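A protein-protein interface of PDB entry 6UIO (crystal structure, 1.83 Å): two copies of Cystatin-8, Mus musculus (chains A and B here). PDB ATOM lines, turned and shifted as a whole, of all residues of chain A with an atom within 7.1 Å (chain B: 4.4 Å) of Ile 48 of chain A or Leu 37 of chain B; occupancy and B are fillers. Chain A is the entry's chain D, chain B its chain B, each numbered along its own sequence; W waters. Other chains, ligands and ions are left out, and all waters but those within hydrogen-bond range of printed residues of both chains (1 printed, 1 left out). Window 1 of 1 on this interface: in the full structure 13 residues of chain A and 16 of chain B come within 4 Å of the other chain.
The backbone carbonyl oxygen (O) of Leu 37 of chain B sits at hydrogen-bond distance from the backbone NH (N) of Ser 61 of chain B (3.0 Å). The side-chain carboxylate of Asp 39 of chain B lies within hydrogen-bond range of the side-chain hydroxyl of Ser 61 of chain B, 2.7 Å away. O of Gly 6 of chain A lies within hydrogen-bond range of N of Leu 46 of chain A. N of Gln 47 of chain A is in hydrogen-bond range of O of Glu 53 of chain A (2.8 Å). OD1 of Asp 50 of chain A is in hydrogen-bond range of OG1 of Thr 49 of chain A, 3.3 Å away. O of Arg 51 of chain A is in hydrogen-bond range of OG1 of Thr 49 of chain A (3.1 Å).
No position is printed for both chains.
Hydrophobic or aromatic side chains of chain A within 4 Å of the printed part of chain B: Tyr 4, Leu 46, Ile 48, Met 52 and Trp 98. Hydrophobic or aromatic side chains of chain B that line the printed part of chain A: Val 19, Trp 20 and Leu 37. Among the printed residues, no Asp or Glu carboxylate lies within 4 Å of a Lys or Arg side-chain nitrogen of the other chain.
Leu 37 of chain B touches three residues of chain A. Of the printed residues of chain A, Val 38 of chain B touches Tyr 4 (3.4 Å). Printed residues of chain B within 4 Å of Met 52 of chain A: Lys 16 and Trp 20. The nearest residue of chain B that does not touch Ile 48 of chain A is Lys 16 of chain B (4.1 Å). The nearest residue of chain A that does not touch Leu 37 of chain B is Gln 47 of chain A (5.6 Å). The nearest printed residue of chain B that does not touch Leu 46 of chain A is Val 38 of chain B (6.8 Å).
Water W1 bridges O of Ile 48 of chain A and N of Val 38 of chain B.
Among the printed residues, pairs that only touch across the chains: Trp 98 of chain A with Trp 20 of chain B (3.2 Å), Thr 49 of chain A with Trp 20 of chain B (3.3 Å), Tyr 4 of chain A with Leu 37 of chain B (3.4 Å), Tyr 4 of chain A with Cys 75 of chain B (3.4 Å), Tyr 4 of chain A with Val 38 of chain B (3.4 Å), Ile 48 of chain A with Leu 37 of chain B (3.4 Å), Tyr 4 of chain A with Asp 39 of chain B (3.4 Å), Tyr 4 of chain A with Ser 63 of chain B (3.5 Å), Ile 48 of chain A with Trp 20 of chain B (3.5 Å), Leu 46 of chain A with Lys 16 of chain B (3.7 Å), Met 52 of chain A with Lys 16 of chain B (3.7 Å), Ile 48 of chain A with Val 19 of chain B (3.9 Å), Gln 47 of chain A with Cys 75 of chain B (3.9 Å), Thr 49 of chain A with Leu 37 of chain B (3.9 Å) and Met 52 of chain A with Trp 20 of chain B (3.9 Å).
The backbone carbonyl oxygen of Asp 50 of chain A lies within hydrogen-bond range of the indole nitrogen of Trp 20 of chain B (3.0 Å). The side-chain hydroxyl (OH) of Tyr 4 of chain A is in hydrogen-bond range of the side-chain hydroxyl (OG) of Ser 61 of chain B.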
ATOM      1  N   TYR A   4      16.571 -18.670 -22.714  1.00  0.00           N
ATOM      2  CA  TYR A   4      16.020 -19.413 -23.871  1.00  0.00           C
ATOM      3  C   TYR A   4      16.308 -18.629 -25.143  1.00  0.00           C
ATOM      4  O   TYR A   4      15.592 -18.819 -26.149  1.00  0.00           O
ATOM      5  CB  TYR A   4      14.533 -19.667 -23.648  1.00  0.00           C
ATOM      6  CG  TYR A   4      14.212 -20.605 -22.519  1.00  0.00           C
ATOM      7  CD1 TYR A   4      14.456 -21.958 -22.628  1.00  0.00           C
ATOM      8  CD2 TYR A   4      13.598 -20.156 -21.365  1.00  0.00           C
ATOM      9  CE1 TYR A   4      14.115 -22.845 -21.626  1.00  0.00           C
ATOM     10  CE2 TYR A   4      13.284 -21.014 -20.332  1.00  0.00           C
ATOM     11  CZ  TYR A   4      13.535 -22.375 -20.461  1.00  0.00           C
ATOM     12  OH  TYR A   4      13.224 -23.259 -19.471  1.00  0.00           O
ATOM     13  N   PHE A   5      17.303 -17.733 -25.109  1.00  0.00           N
ATOM     14  CA  PHE A   5      17.763 -16.994 -26.309  1.00  0.00           C
ATOM     15  C   PHE A   5      18.898 -17.806 -26.924  1.00  0.00           C
ATOM     16  O   PHE A   5      19.785 -18.200 -26.169  1.00  0.00           O
ATOM     17  CB  PHE A   5      18.194 -15.562 -25.993  1.00  0.00           C
ATOM     18  CG  PHE A   5      17.043 -14.611 -25.821  1.00  0.00           C
ATOM     19  CD1 PHE A   5      16.462 -14.413 -24.578  1.00  0.00           C
ATOM     20  CD2 PHE A   5      16.581 -13.877 -26.894  1.00  0.00           C
ATOM     21  CE1 PHE A   5      15.391 -13.550 -24.432  1.00  0.00           C
ATOM     22  CE2 PHE A   5      15.515 -13.009 -26.746  1.00  0.00           C
ATOM     23  CZ  PHE A   5      14.918 -12.857 -25.511  1.00  0.00           C
ATOM     24  N   GLY A   6      18.845 -18.056 -28.245  1.00  0.00           N
ATOM     25  CA  GLY A   6      19.937 -18.700 -29.006  1.00  0.00           C
ATOM     26  C   GLY A   6      20.448 -17.756 -30.087  1.00  0.00           C
ATOM     27  O   GLY A   6      19.634 -17.048 -30.640  1.00  0.00           O
ATOM     28  N   LEU A  46      17.537 -15.203 -30.784  1.00  0.00           N
ATOM     29  CA  LEU A  46      16.107 -15.518 -30.938  1.00  0.00           C
ATOM     30  C   LEU A  46      15.637 -16.342 -29.740  1.00  0.00           C
ATOM     31  O   LEU A  46      16.308 -17.318 -29.371  1.00  0.00           O
ATOM     32  CB  LEU A  46      15.951 -16.318 -32.237  1.00  0.00           C
ATOM     33  CG  LEU A  46      14.637 -17.028 -32.387  1.00  0.00           C
ATOM     34  CD1 LEU A  46      13.527 -16.012 -32.477  1.00  0.00           C
ATOM     35  CD2 LEU A  46      14.678 -17.944 -33.618  1.00  0.00           C
ATOM     36  N   GLN A  47      14.525 -15.936 -29.153  1.00  0.00           N
ATOM     37  CA  GLN A  47      13.790 -16.740 -28.155  1.00  0.00           C
ATOM     38  C   GLN A  47      12.478 -17.149 -28.809  1.00  0.00           C
ATOM     39  O   GLN A  47      11.780 -16.293 -29.332  1.00  0.00           O
ATOM     40  CB  GLN A  47      13.587 -15.972 -26.856  1.00  0.00           C
ATOM     41  CG  GLN A  47      12.729 -16.725 -25.863  1.00  0.00           C
ATOM     42  CD  GLN A  47      12.338 -15.920 -24.653  1.00  0.00           C
ATOM     43  OE1 GLN A  47      12.806 -16.178 -23.561  1.00  0.00           O
ATOM     44  NE2 GLN A  47      11.413 -14.996 -24.830  1.00  0.00           N
ATOM     45  N   ILE A  48      12.166 -18.441 -28.765  1.00  0.00           N
ATOM     46  CA  ILE A  48      10.909 -18.974 -29.354  1.00  0.00           C
ATOM     47  C   ILE A  48       9.920 -19.188 -28.208  1.00  0.00           C
ATOM     48  O   ILE A  48      10.161 -20.069 -27.398  1.00  0.00           O
ATOM     49  CB  ILE A  48      11.198 -20.257 -30.141  1.00  0.00           C
ATOM     50  CG1 ILE A  48      12.163 -19.954 -31.293  1.00  0.00           C
ATOM     51  CG2 ILE A  48       9.907 -20.894 -30.638  1.00  0.00           C
ATOM     52  CD1 ILE A  48      12.638 -21.196 -32.040  1.00  0.00           C
ATOM     53  N   THR A  49       8.863 -18.373 -28.135  1.00  0.00           N
ATOM     54  CA  THR A  49       7.739 -18.596 -27.180  1.00  0.00           C
ATOM     55  C   THR A  49       6.443 -18.612 -27.990  1.00  0.00           C
ATOM     56  O   THR A  49       6.483 -19.107 -29.123  1.00  0.00           O
ATOM     57  CB  THR A  49       7.704 -17.532 -26.074  1.00  0.00           C
ATOM     58  OG1 THR A  49       7.596 -16.277 -26.748  1.00  0.00           O
ATOM     59  CG2 THR A  49       8.917 -17.556 -25.171  1.00  0.00           C
ATOM     60  N   ASP A  50       5.355 -18.016 -27.492  1.00  0.00           N
ATOM     61  CA  ASP A  50       4.096 -17.898 -28.275  1.00  0.00           C
ATOM     62  C   ASP A  50       4.376 -17.022 -29.506  1.00  0.00           C
ATOM     63  O   ASP A  50       3.613 -17.092 -30.456  1.00  0.00           O
ATOM     64  CB  ASP A  50       2.950 -17.349 -27.424  1.00  0.00           C
ATOM     65  CG  ASP A  50       3.190 -15.930 -26.949  1.00  0.00           C
ATOM     66  OD1 ASP A  50       4.340 -15.626 -26.537  1.00  0.00           O
ATOM     67  OD2 ASP A  50       2.246 -15.120 -27.054  1.00  0.00           O
ATOM     68  N   ARG A  51       5.439 -16.218 -29.472  1.00  0.00           N
ATOM     69  CA  ARG A  51       5.917 -15.452 -30.644  1.00  0.00           C
ATOM     70  C   ARG A  51       7.435 -15.611 -30.766  1.00  0.00           C
ATOM     71  O   ARG A  51       8.064 -16.179 -29.838  1.00  0.00           O
ATOM     72  CB  ARG A  51       5.504 -13.984 -30.508  1.00  0.00           C
ATOM     73  CG  ARG A  51       6.270 -13.178 -29.469  1.00  0.00           C
ATOM     74  CD  ARG A  51       5.929 -11.730 -29.718  1.00  0.00           C
ATOM     75  NE  ARG A  51       5.571 -10.974 -28.530  1.00  0.00           N
ATOM     76  CZ  ARG A  51       4.870  -9.854 -28.554  1.00  0.00           C
ATOM     77  NH1 ARG A  51       4.487  -9.322 -29.697  1.00  0.00           N
ATOM     78  NH2 ARG A  51       4.588  -9.263 -27.414  1.00  0.00           N
ATOM     79  N   MET A  52       8.000 -15.119 -31.862  1.00  0.00           N
ATOM     80  CA  MET A  52       9.459 -15.013 -32.032  1.00  0.00           C
ATOM     81  C   MET A  52       9.892 -13.731 -31.343  1.00  0.00           C
ATOM     82  O   MET A  52       9.173 -12.718 -31.525  1.00  0.00           O
ATOM     83  CB  MET A  52       9.832 -14.953 -33.519  1.00  0.00           C
ATOM     84  CG  MET A  52       9.289 -16.124 -34.292  1.00  0.00           C
ATOM     85  SD  MET A  52       9.814 -17.737 -33.628  1.00  0.00           S
ATOM     86  CE  MET A  52      10.863 -18.288 -34.966  1.00  0.00           C
ATOM     87  N   GLU A  53      10.945 -13.786 -30.527  1.00  0.00           N
ATOM     88  CA  GLU A  53      11.533 -12.571 -29.918  1.00  0.00           C
ATOM     89  C   GLU A  53      12.983 -12.481 -30.375  1.00  0.00           C
ATOM     90  O   GLU A  53      13.778 -13.388 -30.051  1.00  0.00           O
ATOM     91  CB  GLU A  53      11.363 -12.562 -28.403  1.00  0.00           C
ATOM     92  CG  GLU A  53       9.930 -12.290 -27.972  1.00  0.00           C
ATOM     93  CD  GLU A  53       9.739 -12.256 -26.465  1.00  0.00           C
ATOM     94  OE1 GLU A  53      10.750 -12.129 -25.761  1.00  0.00           O
ATOM     95  OE2 GLU A  53       8.587 -12.371 -26.007  1.00  0.00           O
ATOM     96  N   TRP A  98       6.047 -14.526 -40.326  1.00  0.00           N
ATOM     97  CA  TRP A  98       5.296 -15.199 -41.420  1.00  0.00           C
ATOM     98  C   TRP A  98       3.949 -14.494 -41.616  1.00  0.00           C
ATOM     99  O   TRP A  98       3.318 -14.733 -42.632  1.00  0.00           O
ATOM    100  CB  TRP A  98       5.110 -16.696 -41.135  1.00  0.00           C
ATOM    101  CG  TRP A  98       4.804 -16.994 -39.695  1.00  0.00           C
ATOM    102  CD1 TRP A  98       3.574 -17.018 -39.103  1.00  0.00           C
ATOM    103  CD2 TRP A  98       5.751 -17.331 -38.667  1.00  0.00           C
ATOM    104  NE1 TRP A  98       3.694 -17.340 -37.779  1.00  0.00           N
ATOM    105  CE2 TRP A  98       5.013 -17.529 -37.482  1.00  0.00           C
ATOM    106  CE3 TRP A  98       7.146 -17.474 -38.631  1.00  0.00           C
ATOM    107  CZ2 TRP A  98       5.619 -17.855 -36.268  1.00  0.00           C
ATOM    108  CZ3 TRP A  98       7.742 -17.819 -37.435  1.00  0.00           C
ATOM    109  CH2 TRP A  98       6.987 -18.004 -36.272  1.00  0.00           C
ATOM    110  N   LYS B  16      13.094 -22.765 -37.962  1.00  0.00           N
ATOM    111  CA  LYS B  16      12.708 -21.947 -36.787  1.00  0.00           C
ATOM    112  C   LYS B  16      11.173 -21.837 -36.712  1.00  0.00           C
ATOM    113  O   LYS B  16      10.675 -21.964 -35.604  1.00  0.00           O
ATOM    114  CB  LYS B  16      13.351 -20.563 -36.805  1.00  0.00           C
ATOM    115  CG  LYS B  16      14.878 -20.527 -36.712  1.00  0.00           C
ATOM    116  CD  LYS B  16      15.444 -21.134 -35.444  1.00  0.00           C
ATOM    117  CE  LYS B  16      16.816 -20.625 -35.045  1.00  0.00           C
ATOM    118  NZ  LYS B  16      17.684 -20.224 -36.179  1.00  0.00           N
ATOM    119  N   VAL B  19       9.866 -25.247 -35.436  1.00  0.00           N
ATOM    120  CA  VAL B  19      10.105 -25.365 -33.966  1.00  0.00           C
ATOM    121  C   VAL B  19       9.078 -24.500 -33.222  1.00  0.00           C
ATOM    122  O   VAL B  19       8.478 -25.005 -32.244  1.00  0.00           O
ATOM    123  CB  VAL B  19      11.546 -24.958 -33.591  1.00  0.00           C
ATOM    124  CG1 VAL B  19      11.736 -24.952 -32.083  1.00  0.00           C
ATOM    125  CG2 VAL B  19      12.587 -25.863 -34.233  1.00  0.00           C
ATOM    126  N   TRP B  20       8.845 -23.255 -33.665  1.00  0.00           N
ATOM    127  CA  TRP B  20       7.796 -22.376 -33.074  1.00  0.00           C
ATOM    128  C   TRP B  20       6.467 -23.126 -33.076  1.00  0.00           C
ATOM    129  O   TRP B  20       5.812 -23.155 -32.074  1.00  0.00           O
ATOM    130  CB  TRP B  20       7.682 -21.053 -33.834  1.00  0.00           C
ATOM    131  CG  TRP B  20       6.467 -20.262 -33.468  1.00  0.00           C
ATOM    132  CD1 TRP B  20       6.280 -19.476 -32.372  1.00  0.00           C
ATOM    133  CD2 TRP B  20       5.226 -20.251 -34.192  1.00  0.00           C
ATOM    134  NE1 TRP B  20       5.000 -18.987 -32.362  1.00  0.00           N
ATOM    135  CE2 TRP B  20       4.336 -19.444 -33.472  1.00  0.00           C
ATOM    136  CE3 TRP B  20       4.783 -20.856 -35.368  1.00  0.00           C
ATOM    137  CZ2 TRP B  20       3.027 -19.224 -33.894  1.00  0.00           C
ATOM    138  CZ3 TRP B  20       3.499 -20.616 -35.798  1.00  0.00           C
ATOM    139  CH2 TRP B  20       2.642 -19.793 -35.080  1.00  0.00           C
ATOM    140  N   MET B  23       6.441 -26.311 -30.692  1.00  0.00           N
ATOM    141  CA  MET B  23       6.485 -25.952 -29.244  1.00  0.00           C
ATOM    142  C   MET B  23       5.149 -25.342 -28.812  1.00  0.00           C
ATOM    143  O   MET B  23       4.695 -25.614 -27.676  1.00  0.00           O
ATOM    144  CB  MET B  23       7.651 -25.005 -28.927  1.00  0.00           C
ATOM    145  CG  MET B  23       9.008 -25.703 -29.010  1.00  0.00           C
ATOM    146  SD  MET B  23       9.119 -27.119 -27.904  1.00  0.00           S
ATOM    147  CE  MET B  23       8.940 -26.342 -26.298  1.00  0.00           C
ATOM    148  N   VAL B  35       5.193 -23.490 -18.768  1.00  0.00           N
ATOM    149  CA  VAL B  35       5.521 -23.503 -20.212  1.00  0.00           C
ATOM    150  C   VAL B  35       6.916 -24.104 -20.372  1.00  0.00           C
ATOM    151  O   VAL B  35       7.752 -23.797 -19.549  1.00  0.00           O
ATOM    152  CB  VAL B  35       5.487 -22.070 -20.760  1.00  0.00           C
ATOM    153  CG1 VAL B  35       6.032 -21.988 -22.164  1.00  0.00           C
ATOM    154  CG2 VAL B  35       4.104 -21.473 -20.675  1.00  0.00           C
ATOM    155  N   PHE B  36       7.135 -24.942 -21.380  1.00  0.00           N
ATOM    156  CA  PHE B  36       8.461 -25.494 -21.719  1.00  0.00           C
ATOM    157  C   PHE B  36       9.026 -24.666 -22.869  1.00  0.00           C
ATOM    158  O   PHE B  36       8.287 -24.452 -23.793  1.00  0.00           O
ATOM    159  CB  PHE B  36       8.388 -26.942 -22.185  1.00  0.00           C
ATOM    160  CG  PHE B  36       8.246 -27.897 -21.044  1.00  0.00           C
ATOM    161  CD1 PHE B  36       7.061 -27.951 -20.357  1.00  0.00           C
ATOM    162  CD2 PHE B  36       9.305 -28.663 -20.608  1.00  0.00           C
ATOM    163  CE1 PHE B  36       6.917 -28.790 -19.279  1.00  0.00           C
ATOM    164  CE2 PHE B  36       9.149 -29.514 -19.532  1.00  0.00           C
ATOM    165  CZ  PHE B  36       7.954 -29.561 -18.866  1.00  0.00           C
ATOM    166  N   LEU B  37      10.275 -24.239 -22.806  1.00  0.00           N
ATOM    167  CA  LEU B  37      10.888 -23.492 -23.916  1.00  0.00           C
ATOM    168  C   LEU B  37      12.132 -24.244 -24.390  1.00  0.00           C
ATOM    169  O   LEU B  37      12.542 -25.181 -23.727  1.00  0.00           O
ATOM    170  CB  LEU B  37      11.183 -22.073 -23.449  1.00  0.00           C
ATOM    171  CG  LEU B  37      10.053 -21.060 -23.483  1.00  0.00           C
ATOM    172  CD1 LEU B  37       8.979 -21.409 -24.488  1.00  0.00           C
ATOM    173  CD2 LEU B  37       9.479 -20.923 -22.109  1.00  0.00           C
ATOM    174  N   VAL B  38      12.666 -23.885 -25.544  1.00  0.00           N
ATOM    175  CA  VAL B  38      13.809 -24.594 -26.167  1.00  0.00           C
ATOM    176  C   VAL B  38      15.168 -24.193 -25.578  1.00  0.00           C
ATOM    177  O   VAL B  38      15.512 -23.028 -25.689  1.00  0.00           O
ATOM    178  CB  VAL B  38      13.825 -24.369 -27.679  1.00  0.00           C
ATOM    179  CG1 VAL B  38      15.025 -25.028 -28.311  1.00  0.00           C
ATOM    180  CG2 VAL B  38      12.547 -24.868 -28.296  1.00  0.00           C
ATOM    181  N   ASP B  39      15.917 -25.141 -25.006  1.00  0.00           N
ATOM    182  CA  ASP B  39      17.308 -24.950 -24.549  1.00  0.00           C
ATOM    183  C   ASP B  39      18.165 -24.860 -25.803  1.00  0.00           C
ATOM    184  O   ASP B  39      19.030 -24.026 -25.822  1.00  0.00           O
ATOM    185  CB  ASP B  39      17.812 -26.107 -23.693  1.00  0.00           C
ATOM    186  CG  ASP B  39      17.209 -26.180 -22.313  1.00  0.00           C
ATOM    187  OD1 ASP B  39      16.565 -25.222 -21.924  1.00  0.00           O
ATOM    188  OD2 ASP B  39      17.393 -27.205 -21.660  1.00  0.00           O
ATOM    189  N   ILE B  60      14.447 -29.253 -24.465  1.00  0.00           N
ATOM    190  CA  ILE B  60      13.505 -28.263 -23.893  1.00  0.00           C
ATOM    191  C   ILE B  60      13.569 -28.369 -22.382  1.00  0.00           C
ATOM    192  O   ILE B  60      13.961 -29.399 -21.880  1.00  0.00           O
ATOM    193  CB  ILE B  60      12.082 -28.512 -24.397  1.00  0.00           C
ATOM    194  CG1 ILE B  60      11.536 -29.833 -23.857  1.00  0.00           C
ATOM    195  CG2 ILE B  60      12.033 -28.463 -25.902  1.00  0.00           C
ATOM    196  CD1 ILE B  60      10.110 -30.080 -24.195  1.00  0.00           C
ATOM    197  N   SER B  61      13.190 -27.325 -21.689  1.00  0.00           N
ATOM    198  CA  SER B  61      13.171 -27.355 -20.221  1.00  0.00           C
ATOM    199  C   SER B  61      11.939 -26.633 -19.672  1.00  0.00           C
ATOM    200  O   SER B  61      11.369 -25.829 -20.368  1.00  0.00           O
ATOM    201  CB  SER B  61      14.448 -26.868 -19.632  1.00  0.00           C
ATOM    202  OG  SER B  61      14.715 -25.554 -20.027  1.00  0.00           O
ATOM    203  N   SER B  63      10.070 -23.956 -17.794  1.00  0.00           N
ATOM    204  CA  SER B  63      10.410 -22.549 -17.487  1.00  0.00           C
ATOM    205  C   SER B  63       9.758 -22.136 -16.174  1.00  0.00           C
ATOM    206  O   SER B  63       9.032 -22.940 -15.607  1.00  0.00           O
ATOM    207  CB  SER B  63       9.952 -21.655 -18.581  1.00  0.00           C
ATOM    208  OG  SER B  63       8.605 -21.298 -18.396  1.00  0.00           O
ATOM    209  N   CYS B  75      10.938 -15.373 -19.033  1.00  0.00           N
ATOM    210  CA  CYS B  75      10.925 -16.836 -18.795  1.00  0.00           C
ATOM    211  C   CYS B  75      12.357 -17.410 -18.814  1.00  0.00           C
ATOM    212  O   CYS B  75      13.043 -17.178 -19.800  1.00  0.00           O
ATOM    213  CB  CYS B  75      10.076 -17.544 -19.838  1.00  0.00           C
ATOM    214  SG  CYS B  75       8.364 -16.963 -19.886  1.00  0.00           S
HETATM  215  O   HOH W   1      12.248 -21.307 -26.378  1.00  0.00           O
